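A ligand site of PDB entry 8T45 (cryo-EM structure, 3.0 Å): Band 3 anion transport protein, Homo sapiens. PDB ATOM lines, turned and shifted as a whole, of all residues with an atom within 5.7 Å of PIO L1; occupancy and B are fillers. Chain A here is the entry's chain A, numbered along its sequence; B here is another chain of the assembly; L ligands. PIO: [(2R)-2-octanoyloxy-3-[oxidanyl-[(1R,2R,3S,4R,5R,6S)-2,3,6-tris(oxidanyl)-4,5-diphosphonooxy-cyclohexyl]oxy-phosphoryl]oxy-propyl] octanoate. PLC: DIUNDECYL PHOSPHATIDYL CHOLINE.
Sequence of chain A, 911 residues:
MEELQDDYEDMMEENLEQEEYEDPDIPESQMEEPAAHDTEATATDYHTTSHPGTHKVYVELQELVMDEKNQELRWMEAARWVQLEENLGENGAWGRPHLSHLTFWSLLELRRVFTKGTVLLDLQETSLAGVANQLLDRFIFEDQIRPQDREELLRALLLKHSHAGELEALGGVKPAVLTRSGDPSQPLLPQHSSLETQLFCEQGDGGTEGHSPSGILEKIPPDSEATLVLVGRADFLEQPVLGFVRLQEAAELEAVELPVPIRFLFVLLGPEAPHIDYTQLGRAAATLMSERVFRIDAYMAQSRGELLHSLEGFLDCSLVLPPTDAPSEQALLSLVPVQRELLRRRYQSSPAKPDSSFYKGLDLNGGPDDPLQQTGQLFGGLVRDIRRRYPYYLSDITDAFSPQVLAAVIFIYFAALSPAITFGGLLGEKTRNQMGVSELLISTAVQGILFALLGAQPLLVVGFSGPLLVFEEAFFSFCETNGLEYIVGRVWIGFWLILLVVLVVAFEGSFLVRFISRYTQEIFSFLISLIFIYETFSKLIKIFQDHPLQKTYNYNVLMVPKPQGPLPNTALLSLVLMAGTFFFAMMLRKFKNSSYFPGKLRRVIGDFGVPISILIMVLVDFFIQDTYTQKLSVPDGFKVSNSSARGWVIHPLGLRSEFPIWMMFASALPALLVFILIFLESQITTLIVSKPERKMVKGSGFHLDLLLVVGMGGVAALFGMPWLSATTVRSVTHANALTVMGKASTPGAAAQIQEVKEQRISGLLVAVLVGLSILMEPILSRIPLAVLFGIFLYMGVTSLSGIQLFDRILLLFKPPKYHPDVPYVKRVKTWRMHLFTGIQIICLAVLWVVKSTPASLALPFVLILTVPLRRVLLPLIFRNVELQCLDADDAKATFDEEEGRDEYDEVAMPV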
ATOM      1  N   PHE A 597     -28.377  -1.902  -7.637  1.00  0.00           N
ATOM      2  CA  PHE A 597     -29.419  -2.931  -7.594  1.00  0.00           C
ATOM      3  C   PHE A 597     -28.817  -4.299  -7.274  1.00  0.00           C
ATOM      4  O   PHE A 597     -27.590  -4.464  -7.326  1.00  0.00           O
ATOM      5  CB  PHE A 597     -30.186  -2.959  -8.917  1.00  0.00           C
ATOM      6  CG  PHE A 597     -31.263  -1.915  -9.020  1.00  0.00           C
ATOM      7  CD1 PHE A 597     -30.926  -0.590  -9.184  1.00  0.00           C
ATOM      8  CD2 PHE A 597     -32.598  -2.270  -8.951  1.00  0.00           C
ATOM      9  CE1 PHE A 597     -31.910   0.384  -9.275  1.00  0.00           C
ATOM     10  CE2 PHE A 597     -33.581  -1.308  -9.034  1.00  0.00           C
ATOM     11  CZ  PHE A 597     -33.238   0.025  -9.199  1.00  0.00           C
ATOM     12  N   PRO A 598     -29.634  -5.289  -6.906  1.00  0.00           N
ATOM     13  CA  PRO A 598     -29.091  -6.633  -6.668  1.00  0.00           C
ATOM     14  C   PRO A 598     -28.408  -7.192  -7.912  1.00  0.00           C
ATOM     15  O   PRO A 598     -28.822  -6.916  -9.040  1.00  0.00           O
ATOM     16  CB  PRO A 598     -30.320  -7.456  -6.283  1.00  0.00           C
ATOM     17  CG  PRO A 598     -31.277  -6.458  -5.743  1.00  0.00           C
ATOM     18  CD  PRO A 598     -31.045  -5.200  -6.518  1.00  0.00           C
ATOM     19  N   GLY A 599     -27.354  -7.965  -7.681  1.00  0.00           N
ATOM     20  CA  GLY A 599     -26.535  -8.440  -8.786  1.00  0.00           C
ATOM     21  C   GLY A 599     -27.322  -9.266  -9.791  1.00  0.00           C
ATOM     22  O   GLY A 599     -27.145  -9.107 -11.007  1.00  0.00           O
ATOM     23  N   LYS A 600     -28.181 -10.157  -9.311  1.00  0.00           N
ATOM     24  CA  LYS A 600     -28.999 -10.967 -10.215  1.00  0.00           C
ATOM     25  C   LYS A 600     -29.926 -10.095 -11.038  1.00  0.00           C
ATOM     26  O   LYS A 600     -30.004 -10.234 -12.275  1.00  0.00           O
ATOM     27  CB  LYS A 600     -29.790 -12.008  -9.415  1.00  0.00           C
ATOM     28  CG  LYS A 600     -30.849 -12.737 -10.227  1.00  0.00           C
ATOM     29  CD  LYS A 600     -32.250 -12.300  -9.825  1.00  0.00           C
ATOM     30  CE  LYS A 600     -33.266 -12.624 -10.902  1.00  0.00           C
ATOM     31  NZ  LYS A 600     -34.585 -11.968 -10.654  1.00  0.00           N
ATOM     32  N   LEU A 601     -30.659  -9.195 -10.375  1.00  0.00           N
ATOM     33  CA  LEU A 601     -31.569  -8.313 -11.094  1.00  0.00           C
ATOM     34  C   LEU A 601     -30.815  -7.387 -12.039  1.00  0.00           C
ATOM     35  O   LEU A 601     -31.248  -7.161 -13.174  1.00  0.00           O
ATOM     36  CB  LEU A 601     -32.405  -7.497 -10.098  1.00  0.00           C
ATOM     37  CG  LEU A 601     -33.591  -6.733 -10.684  1.00  0.00           C
ATOM     38  CD1 LEU A 601     -34.830  -6.956  -9.830  1.00  0.00           C
ATOM     39  CD2 LEU A 601     -33.272  -5.256 -10.816  1.00  0.00           C
ATOM     40  N   ARG A 602     -29.681  -6.855 -11.595  1.00  0.00           N
ATOM     41  CA  ARG A 602     -28.885  -5.989 -12.459  1.00  0.00           C
ATOM     42  C   ARG A 602     -28.413  -6.724 -13.704  1.00  0.00           C
ATOM     43  O   ARG A 602     -28.495  -6.190 -14.811  1.00  0.00           O
ATOM     44  CB  ARG A 602     -27.688  -5.442 -11.674  1.00  0.00           C
ATOM     45  CG  ARG A 602     -26.561  -4.903 -12.535  1.00  0.00           C
ATOM     46  CD  ARG A 602     -25.554  -4.145 -11.691  1.00  0.00           C
ATOM     47  NE  ARG A 602     -24.529  -5.017 -11.144  1.00  0.00           N
ATOM     48  CZ  ARG A 602     -24.453  -5.366  -9.864  1.00  0.00           C
ATOM     49  NH1 ARG A 602     -25.343  -4.950  -8.979  1.00  0.00           N
ATOM     50  NH2 ARG A 602     -23.467  -6.169  -9.465  1.00  0.00           N
ATOM     51  N   ARG A 603     -27.941  -7.964 -13.536  1.00  0.00           N
ATOM     52  CA  ARG A 603     -27.447  -8.718 -14.683  1.00  0.00           C
ATOM     53  C   ARG A 603     -28.565  -9.096 -15.633  1.00  0.00           C
ATOM     54  O   ARG A 603     -28.396  -9.032 -16.864  1.00  0.00           O
ATOM     55  CB  ARG A 603     -26.686  -9.951 -14.202  1.00  0.00           C
ATOM     56  CG  ARG A 603     -25.300  -9.654 -13.671  1.00  0.00           C
ATOM     57  CD  ARG A 603     -24.514 -10.922 -13.396  1.00  0.00           C
ATOM     58  NE  ARG A 603     -24.995 -11.617 -12.220  1.00  0.00           N
ATOM     59  CZ  ARG A 603     -24.557 -11.400 -10.987  1.00  0.00           C
ATOM     60  NH1 ARG A 603     -23.620 -10.499 -10.738  1.00  0.00           N
ATOM     61  NH2 ARG A 603     -25.064 -12.113  -9.979  1.00  0.00           N
ATOM     62  N   LEU B 811     -26.292   5.508  -2.751  1.00  0.00           N
ATOM     63  CA  LEU B 811     -25.995   4.316  -1.959  1.00  0.00           C
ATOM     64  C   LEU B 811     -27.258   3.590  -1.507  1.00  0.00           C
ATOM     65  O   LEU B 811     -27.196   2.392  -1.214  1.00  0.00           O
ATOM     66  CB  LEU B 811     -25.154   4.689  -0.737  1.00  0.00           C
ATOM     67  CG  LEU B 811     -23.740   5.178  -1.028  1.00  0.00           C
ATOM     68  CD1 LEU B 811     -22.917   5.222   0.253  1.00  0.00           C
ATOM     69  CD2 LEU B 811     -23.079   4.298  -2.068  1.00  0.00           C
ATOM     70  N   LEU B 812     -28.386   4.291  -1.434  1.00  0.00           N
ATOM     71  CA  LEU B 812     -29.647   3.630  -1.132  1.00  0.00           C
ATOM     72  C   LEU B 812     -29.941   2.506  -2.113  1.00  0.00           C
ATOM     73  O   LEU B 812     -30.607   1.523  -1.758  1.00  0.00           O
ATOM     74  CB  LEU B 812     -30.804   4.637  -1.142  1.00  0.00           C
ATOM     75  CG  LEU B 812     -31.055   5.472   0.114  1.00  0.00           C
ATOM     76  CD1 LEU B 812     -31.926   6.661  -0.224  1.00  0.00           C
ATOM     77  CD2 LEU B 812     -31.690   4.630   1.202  1.00  0.00           C
ATOM     78  N   PHE B 813     -29.460   2.630  -3.351  1.00  0.00           N
ATOM     79  CA  PHE B 813     -29.684   1.619  -4.383  1.00  0.00           C
ATOM     80  C   PHE B 813     -28.547   0.621  -4.514  1.00  0.00           C
ATOM     81  O   PHE B 813     -28.777  -0.500  -4.972  1.00  0.00           O
ATOM     82  CB  PHE B 813     -29.917   2.300  -5.741  1.00  0.00           C
ATOM     83  CG  PHE B 813     -31.015   3.322  -5.729  1.00  0.00           C
ATOM     84  CD1 PHE B 813     -32.342   2.940  -5.703  1.00  0.00           C
ATOM     85  CD2 PHE B 813     -30.712   4.678  -5.728  1.00  0.00           C
ATOM     86  CE1 PHE B 813     -33.349   3.878  -5.685  1.00  0.00           C
ATOM     87  CE2 PHE B 813     -31.719   5.616  -5.710  1.00  0.00           C
ATOM     88  CZ  PHE B 813     -33.040   5.218  -5.685  1.00  0.00           C
ATOM     89  N   LYS B 814     -27.331   1.001  -4.130  1.00  0.00           N
ATOM     90  CA  LYS B 814     -26.215   0.067  -4.194  1.00  0.00           C
ATOM     91  C   LYS B 814     -26.308  -0.957  -3.072  1.00  0.00           C
ATOM     92  O   LYS B 814     -26.764  -0.637  -1.966  1.00  0.00           O
ATOM     93  CB  LYS B 814     -24.882   0.811  -4.090  1.00  0.00           C
ATOM     94  CG  LYS B 814     -24.541   1.665  -5.302  1.00  0.00           C
ATOM     95  CD  LYS B 814     -23.137   2.220  -5.180  1.00  0.00           C
ATOM     96  CE  LYS B 814     -22.783   3.096  -6.360  1.00  0.00           C
ATOM     97  NZ  LYS B 814     -21.485   3.800  -6.151  1.00  0.00           N
ATOM     98  N   PRO B 815     -25.899  -2.204  -3.324  1.00  0.00           N
ATOM     99  CA  PRO B 815     -25.811  -3.172  -2.237  1.00  0.00           C
ATOM    100  C   PRO B 815     -24.760  -2.740  -1.239  1.00  0.00           C
ATOM    101  O   PRO B 815     -23.799  -2.036  -1.587  1.00  0.00           O
ATOM    102  CB  PRO B 815     -25.428  -4.471  -2.952  1.00  0.00           C
ATOM    103  CG  PRO B 815     -25.894  -4.288  -4.346  1.00  0.00           C
ATOM    104  CD  PRO B 815     -25.710  -2.839  -4.636  1.00  0.00           C
ATOM    105  N   PRO B 816     -24.906  -3.141   0.027  1.00  0.00           N
ATOM    106  CA  PRO B 816     -23.960  -2.669   1.060  1.00  0.00           C
ATOM    107  C   PRO B 816     -22.514  -3.025   0.788  1.00  0.00           C
ATOM    108  O   PRO B 816     -21.614  -2.322   1.253  1.00  0.00           O
ATOM    109  CB  PRO B 816     -24.484  -3.340   2.338  1.00  0.00           C
ATOM    110  CG  PRO B 816     -25.924  -3.596   2.070  1.00  0.00           C
ATOM    111  CD  PRO B 816     -26.008  -3.935   0.613  1.00  0.00           C
ATOM    112  N   LYS B 817     -22.248  -4.115   0.058  1.00  0.00           N
ATOM    113  CA  LYS B 817     -20.872  -4.478  -0.234  1.00  0.00           C
ATOM    114  C   LYS B 817     -20.222  -3.485  -1.196  1.00  0.00           C
ATOM    115  O   LYS B 817     -18.992  -3.367  -1.214  1.00  0.00           O
ATOM    116  CB  LYS B 817     -20.799  -5.896  -0.808  1.00  0.00           C
ATOM    117  CG  LYS B 817     -21.928  -6.241  -1.757  1.00  0.00           C
ATOM    118  CD  LYS B 817     -21.590  -7.461  -2.590  1.00  0.00           C
ATOM    119  CE  LYS B 817     -20.233  -7.317  -3.262  1.00  0.00           C
ATOM    120  NZ  LYS B 817     -19.865  -8.514  -4.067  1.00  0.00           N
ATOM    121  N   TYR B 818     -21.014  -2.785  -2.003  1.00  0.00           N
ATOM    122  CA  TYR B 818     -20.490  -1.833  -2.971  1.00  0.00           C
ATOM    123  C   TYR B 818     -20.372  -0.423  -2.416  1.00  0.00           C
ATOM    124  O   TYR B 818     -19.980   0.493  -3.157  1.00  0.00           O
ATOM    125  CB  TYR B 818     -21.373  -1.820  -4.226  1.00  0.00           C
ATOM    126  CG  TYR B 818     -21.321  -3.110  -5.021  1.00  0.00           C
ATOM    127  CD1 TYR B 818     -20.210  -3.418  -5.787  1.00  0.00           C
ATOM    128  CD2 TYR B 818     -22.382  -3.997  -5.004  1.00  0.00           C
ATOM    129  CE1 TYR B 818     -20.156  -4.599  -6.515  1.00  0.00           C
ATOM    130  CE2 TYR B 818     -22.333  -5.174  -5.724  1.00  0.00           C
ATOM    131  CZ  TYR B 818     -21.225  -5.464  -6.476  1.00  0.00           C
ATOM    132  OH  TYR B 818     -21.183  -6.637  -7.203  1.00  0.00           O
ATOM    133  N   HIS B 834     -29.253   4.842   6.053  1.00  0.00           N
ATOM    134  CA  HIS B 834     -30.434   4.930   5.215  1.00  0.00           C
ATOM    135  C   HIS B 834     -31.562   5.683   5.901  1.00  0.00           C
ATOM    136  O   HIS B 834     -32.320   6.392   5.246  1.00  0.00           O
ATOM    137  CB  HIS B 834     -30.890   3.533   4.815  1.00  0.00           C
ATOM    138  CG  HIS B 834     -30.029   2.895   3.760  1.00  0.00           C
ATOM    139  ND1 HIS B 834     -29.035   3.588   3.109  1.00  0.00           N
ATOM    140  CD2 HIS B 834     -30.021   1.642   3.249  1.00  0.00           C
ATOM    141  CE1 HIS B 834     -28.449   2.781   2.241  1.00  0.00           C
ATOM    142  NE2 HIS B 834     -29.031   1.596   2.299  1.00  0.00           N
HETATM  143  C1  PIO L   1     -26.679  -8.873  -2.891  1.00  0.00           C
HETATM  144  O1  PIO L   1     -26.380  -8.351  -1.623  1.00  0.00           O
HETATM  145  P1  PIO L   1     -27.579  -7.655  -0.729  1.00  0.00           P
HETATM  146  C2  PIO L   1     -26.684 -10.411  -2.810  1.00  0.00           C
HETATM  147  O2  PIO L   1     -27.529 -10.806  -1.766  1.00  0.00           O
HETATM  148  C3  PIO L   1     -25.286 -11.007  -2.571  1.00  0.00           C
HETATM  149  O3  PIO L   1     -25.033 -11.004  -1.191  1.00  0.00           O
HETATM  150  C4  PIO L   1     -24.157 -10.249  -3.300  1.00  0.00           C
HETATM  151  O4  PIO L   1     -23.268 -11.180  -3.851  1.00  0.00           O
HETATM  152  P4  PIO L   1     -22.230 -11.979  -2.846  1.00  0.00           P
HETATM  153  C5  PIO L   1     -24.691  -9.359  -4.429  1.00  0.00           C
HETATM  154  O5  PIO L   1     -23.602  -8.693  -5.027  1.00  0.00           O
HETATM  155  P5  PIO L   1     -23.147  -9.156  -6.545  1.00  0.00           P
HETATM  156  C6  PIO L   1     -25.676  -8.308  -3.907  1.00  0.00           C
HETATM  157  O6  PIO L   1     -26.389  -7.793  -5.011  1.00  0.00           O
HETATM  158  O11 PIO L   1     -27.057  -7.331   0.653  1.00  0.00           O
HETATM  159  O12 PIO L   1     -28.731  -8.621  -0.614  1.00  0.00           O
HETATM  160  O13 PIO L   1     -28.102  -6.266  -1.460  1.00  0.00           O
HETATM  161  C1A PIO L   1     -29.746  -2.779  -2.649  1.00  0.00           C
HETATM  162  O1A PIO L   1     -29.411  -1.723  -2.224  1.00  0.00           O
HETATM  163  C1B PIO L   1     -33.187  -5.949  -0.901  1.00  0.00           C
HETATM  164  O1B PIO L   1     -33.661  -6.421   0.079  1.00  0.00           O
HETATM  165  C1C PIO L   1     -29.188  -6.344  -2.332  1.00  0.00           C
HETATM  166  C2A PIO L   1     -30.738  -2.834  -3.811  1.00  0.00           C
HETATM  167  C2B PIO L   1     -34.011  -5.024  -1.786  1.00  0.00           C
HETATM  168  C2C PIO L   1     -30.040  -5.080  -2.236  1.00  0.00           C
HETATM  169  O2C PIO L   1     -29.215  -3.957  -2.105  1.00  0.00           O
HETATM  170  C3A PIO L   1     -31.872  -1.838  -3.565  1.00  0.00           C
HETATM  171  C3B PIO L   1     -34.937  -5.856  -2.673  1.00  0.00           C
HETATM  172  C3C PIO L   1     -30.973  -5.179  -1.037  1.00  0.00           C
HETATM  173  O3C PIO L   1     -31.865  -6.238  -1.251  1.00  0.00           O
HETATM  174  O41 PIO L   1     -22.806 -13.329  -2.504  1.00  0.00           O
HETATM  175  O42 PIO L   1     -22.036 -11.182  -1.585  1.00  0.00           O
HETATM  176  O43 PIO L   1     -20.897 -12.163  -3.538  1.00  0.00           O
HETATM  177  C4A PIO L   1     -32.759  -1.759  -4.809  1.00  0.00           C
HETATM  178  C4B PIO L   1     -35.451  -5.007  -3.818  1.00  0.00           C
HETATM  179  O51 PIO L   1     -21.656  -9.372  -6.581  1.00  0.00           O
HETATM  180  O52 PIO L   1     -23.844 -10.447  -6.905  1.00  0.00           O
HETATM  181  O53 PIO L   1     -23.527  -8.083  -7.530  1.00  0.00           O
HETATM  182  C5A PIO L   1     -34.137  -1.233  -4.431  1.00  0.00           C
HETATM  183  C5B PIO L   1     -35.528  -5.858  -5.088  1.00  0.00           C
HETATM  184  C6B PIO L   1     -35.434  -4.954  -6.320  1.00  0.00           C
HETATM  185  C7B PIO L   1     -36.769  -4.249  -6.536  1.00  0.00           C
HETATM  186  C8B PIO L   1     -36.611  -3.189  -7.631  1.00  0.00           C
HETATM  187  C1  PLC L   2     -30.212  -2.852   4.452  1.00  0.00           C
HETATM  188  C2  PLC L   2     -31.244  -1.843   3.963  1.00  0.00           C
HETATM  189  C3  PLC L   2     -31.420  -1.776   2.461  1.00  0.00           C
HETATM  190  C'  PLC L   2     -32.929  -1.426   5.612  1.00  0.00           C
HETATM  191  C1' PLC L   2     -32.750   0.062   5.438  1.00  0.00           C
HETATM  192  C2' PLC L   2     -34.060   0.832   5.438  1.00  0.00           C
HETATM  193  C3' PLC L   2     -33.957   2.119   6.242  1.00  0.00           C
HETATM  194  C4' PLC L   2     -35.029   3.141   5.864  1.00  0.00           C
HETATM  195  C5' PLC L   2     -35.101   3.382   4.357  1.00  0.00           C
HETATM  196  C6' PLC L   2     -35.762   4.692   3.987  1.00  0.00           C
HETATM  197  C7' PLC L   2     -35.756   4.955   2.484  1.00  0.00           C
HETATM  198  C8' PLC L   2     -36.212   6.360   2.107  1.00  0.00           C
HETATM  199  C9' PLC L   2     -37.583   6.724   2.666  1.00  0.00           C
HETATM  200  CA' PLC L   2     -38.106   8.059   2.141  1.00  0.00           C
HETATM  201  CB' PLC L   2     -39.450   8.438   2.744  1.00  0.00           C
HETATM  202  CB  PLC L   2     -32.593  -0.525   0.844  1.00  0.00           C
HETATM  203  C1B PLC L   2     -33.497   0.666   0.651  1.00  0.00           C
HETATM  204  C2B PLC L   2     -33.888   0.910  -0.799  1.00  0.00           C
HETATM  205  C3B PLC L   2     -34.891   2.044  -0.938  1.00  0.00           C
HETATM  206  C4B PLC L   2     -35.193   2.388  -2.385  1.00  0.00           C
HETATM  207  O'  PLC L   2     -33.378  -1.950   6.597  1.00  0.00           O
HETATM  208  OB  PLC L   2     -32.166  -1.231  -0.038  1.00  0.00           O
HETATM  209  O2  PLC L   2     -32.521  -2.097   4.537  1.00  0.00           O
HETATM  210  O3  PLC L   2     -32.300  -0.715   2.125  1.00  0.00           O
HETATM  211  O1P PLC L   2     -28.833  -3.156   7.870  1.00  0.00           O
HETATM  212  O2P PLC L   2     -28.101  -4.287   5.646  1.00  0.00           O
HETATM  213  O3P PLC L   2     -30.407  -3.126   5.823  1.00  0.00           O
HETATM  214  O4P PLC L   2     -30.104  -5.211   6.962  1.00  0.00           O
HETATM  215  P   PLC L   2     -29.187  -3.883   6.611  1.00  0.00           P
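NH2 of Arg 602 is in salt-bridge range of O53 of PIO L1 (2.7 Å). The side-chain hydroxyl of Tyr 818 of chain B is in hydrogen-bond range of an oxygen (O53) of PIO L1, at 2.8 Å. The backbone NH of Gly 599 is in hydrogen-bond range of an oxygen (O6) of PIO L1 (2.8 Å). The side-chain amino group (NZ) of Lys 817 of chain B lies within salt-bridge range of an oxygen (O51) of PIO L1 (3.2 Å). The guanidinium group of Arg 603 lies within salt-bridge range of an oxygen (O52) of PIO L1 (3.7 Å).
OH of Tyr 818 of chain B lies within hydrogen-bond range of NH2 of Arg 602 (3.2 Å). The backbone carbonyl oxygen (O) of Phe 597 is in hydrogen-bond range of the guanidinium group (NH1) of Arg 602, 2.8 Å away. The backbone carbonyl oxygen of Phe 813 of chain B lies within hydrogen-bond range of the backbone NH of Phe 597, at 3.0 Å.
O of Leu 812 of chain B lies close to O1A of PIO L1, 3.5 Å away. O1A of PIO L1 sits close to O of Phe 813 of chain B (3.1 Å). O of Lys 814 of chain B sits close to O1A of PIO L1, at 2.9 Å. CE2 of Phe 597 touches C8B of PIO L1, at 3.8 Å. Pro 598 touches PIO L1. Pro 815 of chain B touches PIO L1. Pro 816 of chain B touches PIO L1. Hydrophobic or aromatic side chains within 4 Å of PIO L1: Phe 597, Pro 598, Pro 815 of chain B, Pro 816 of chain B and Tyr 818 of chain B.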
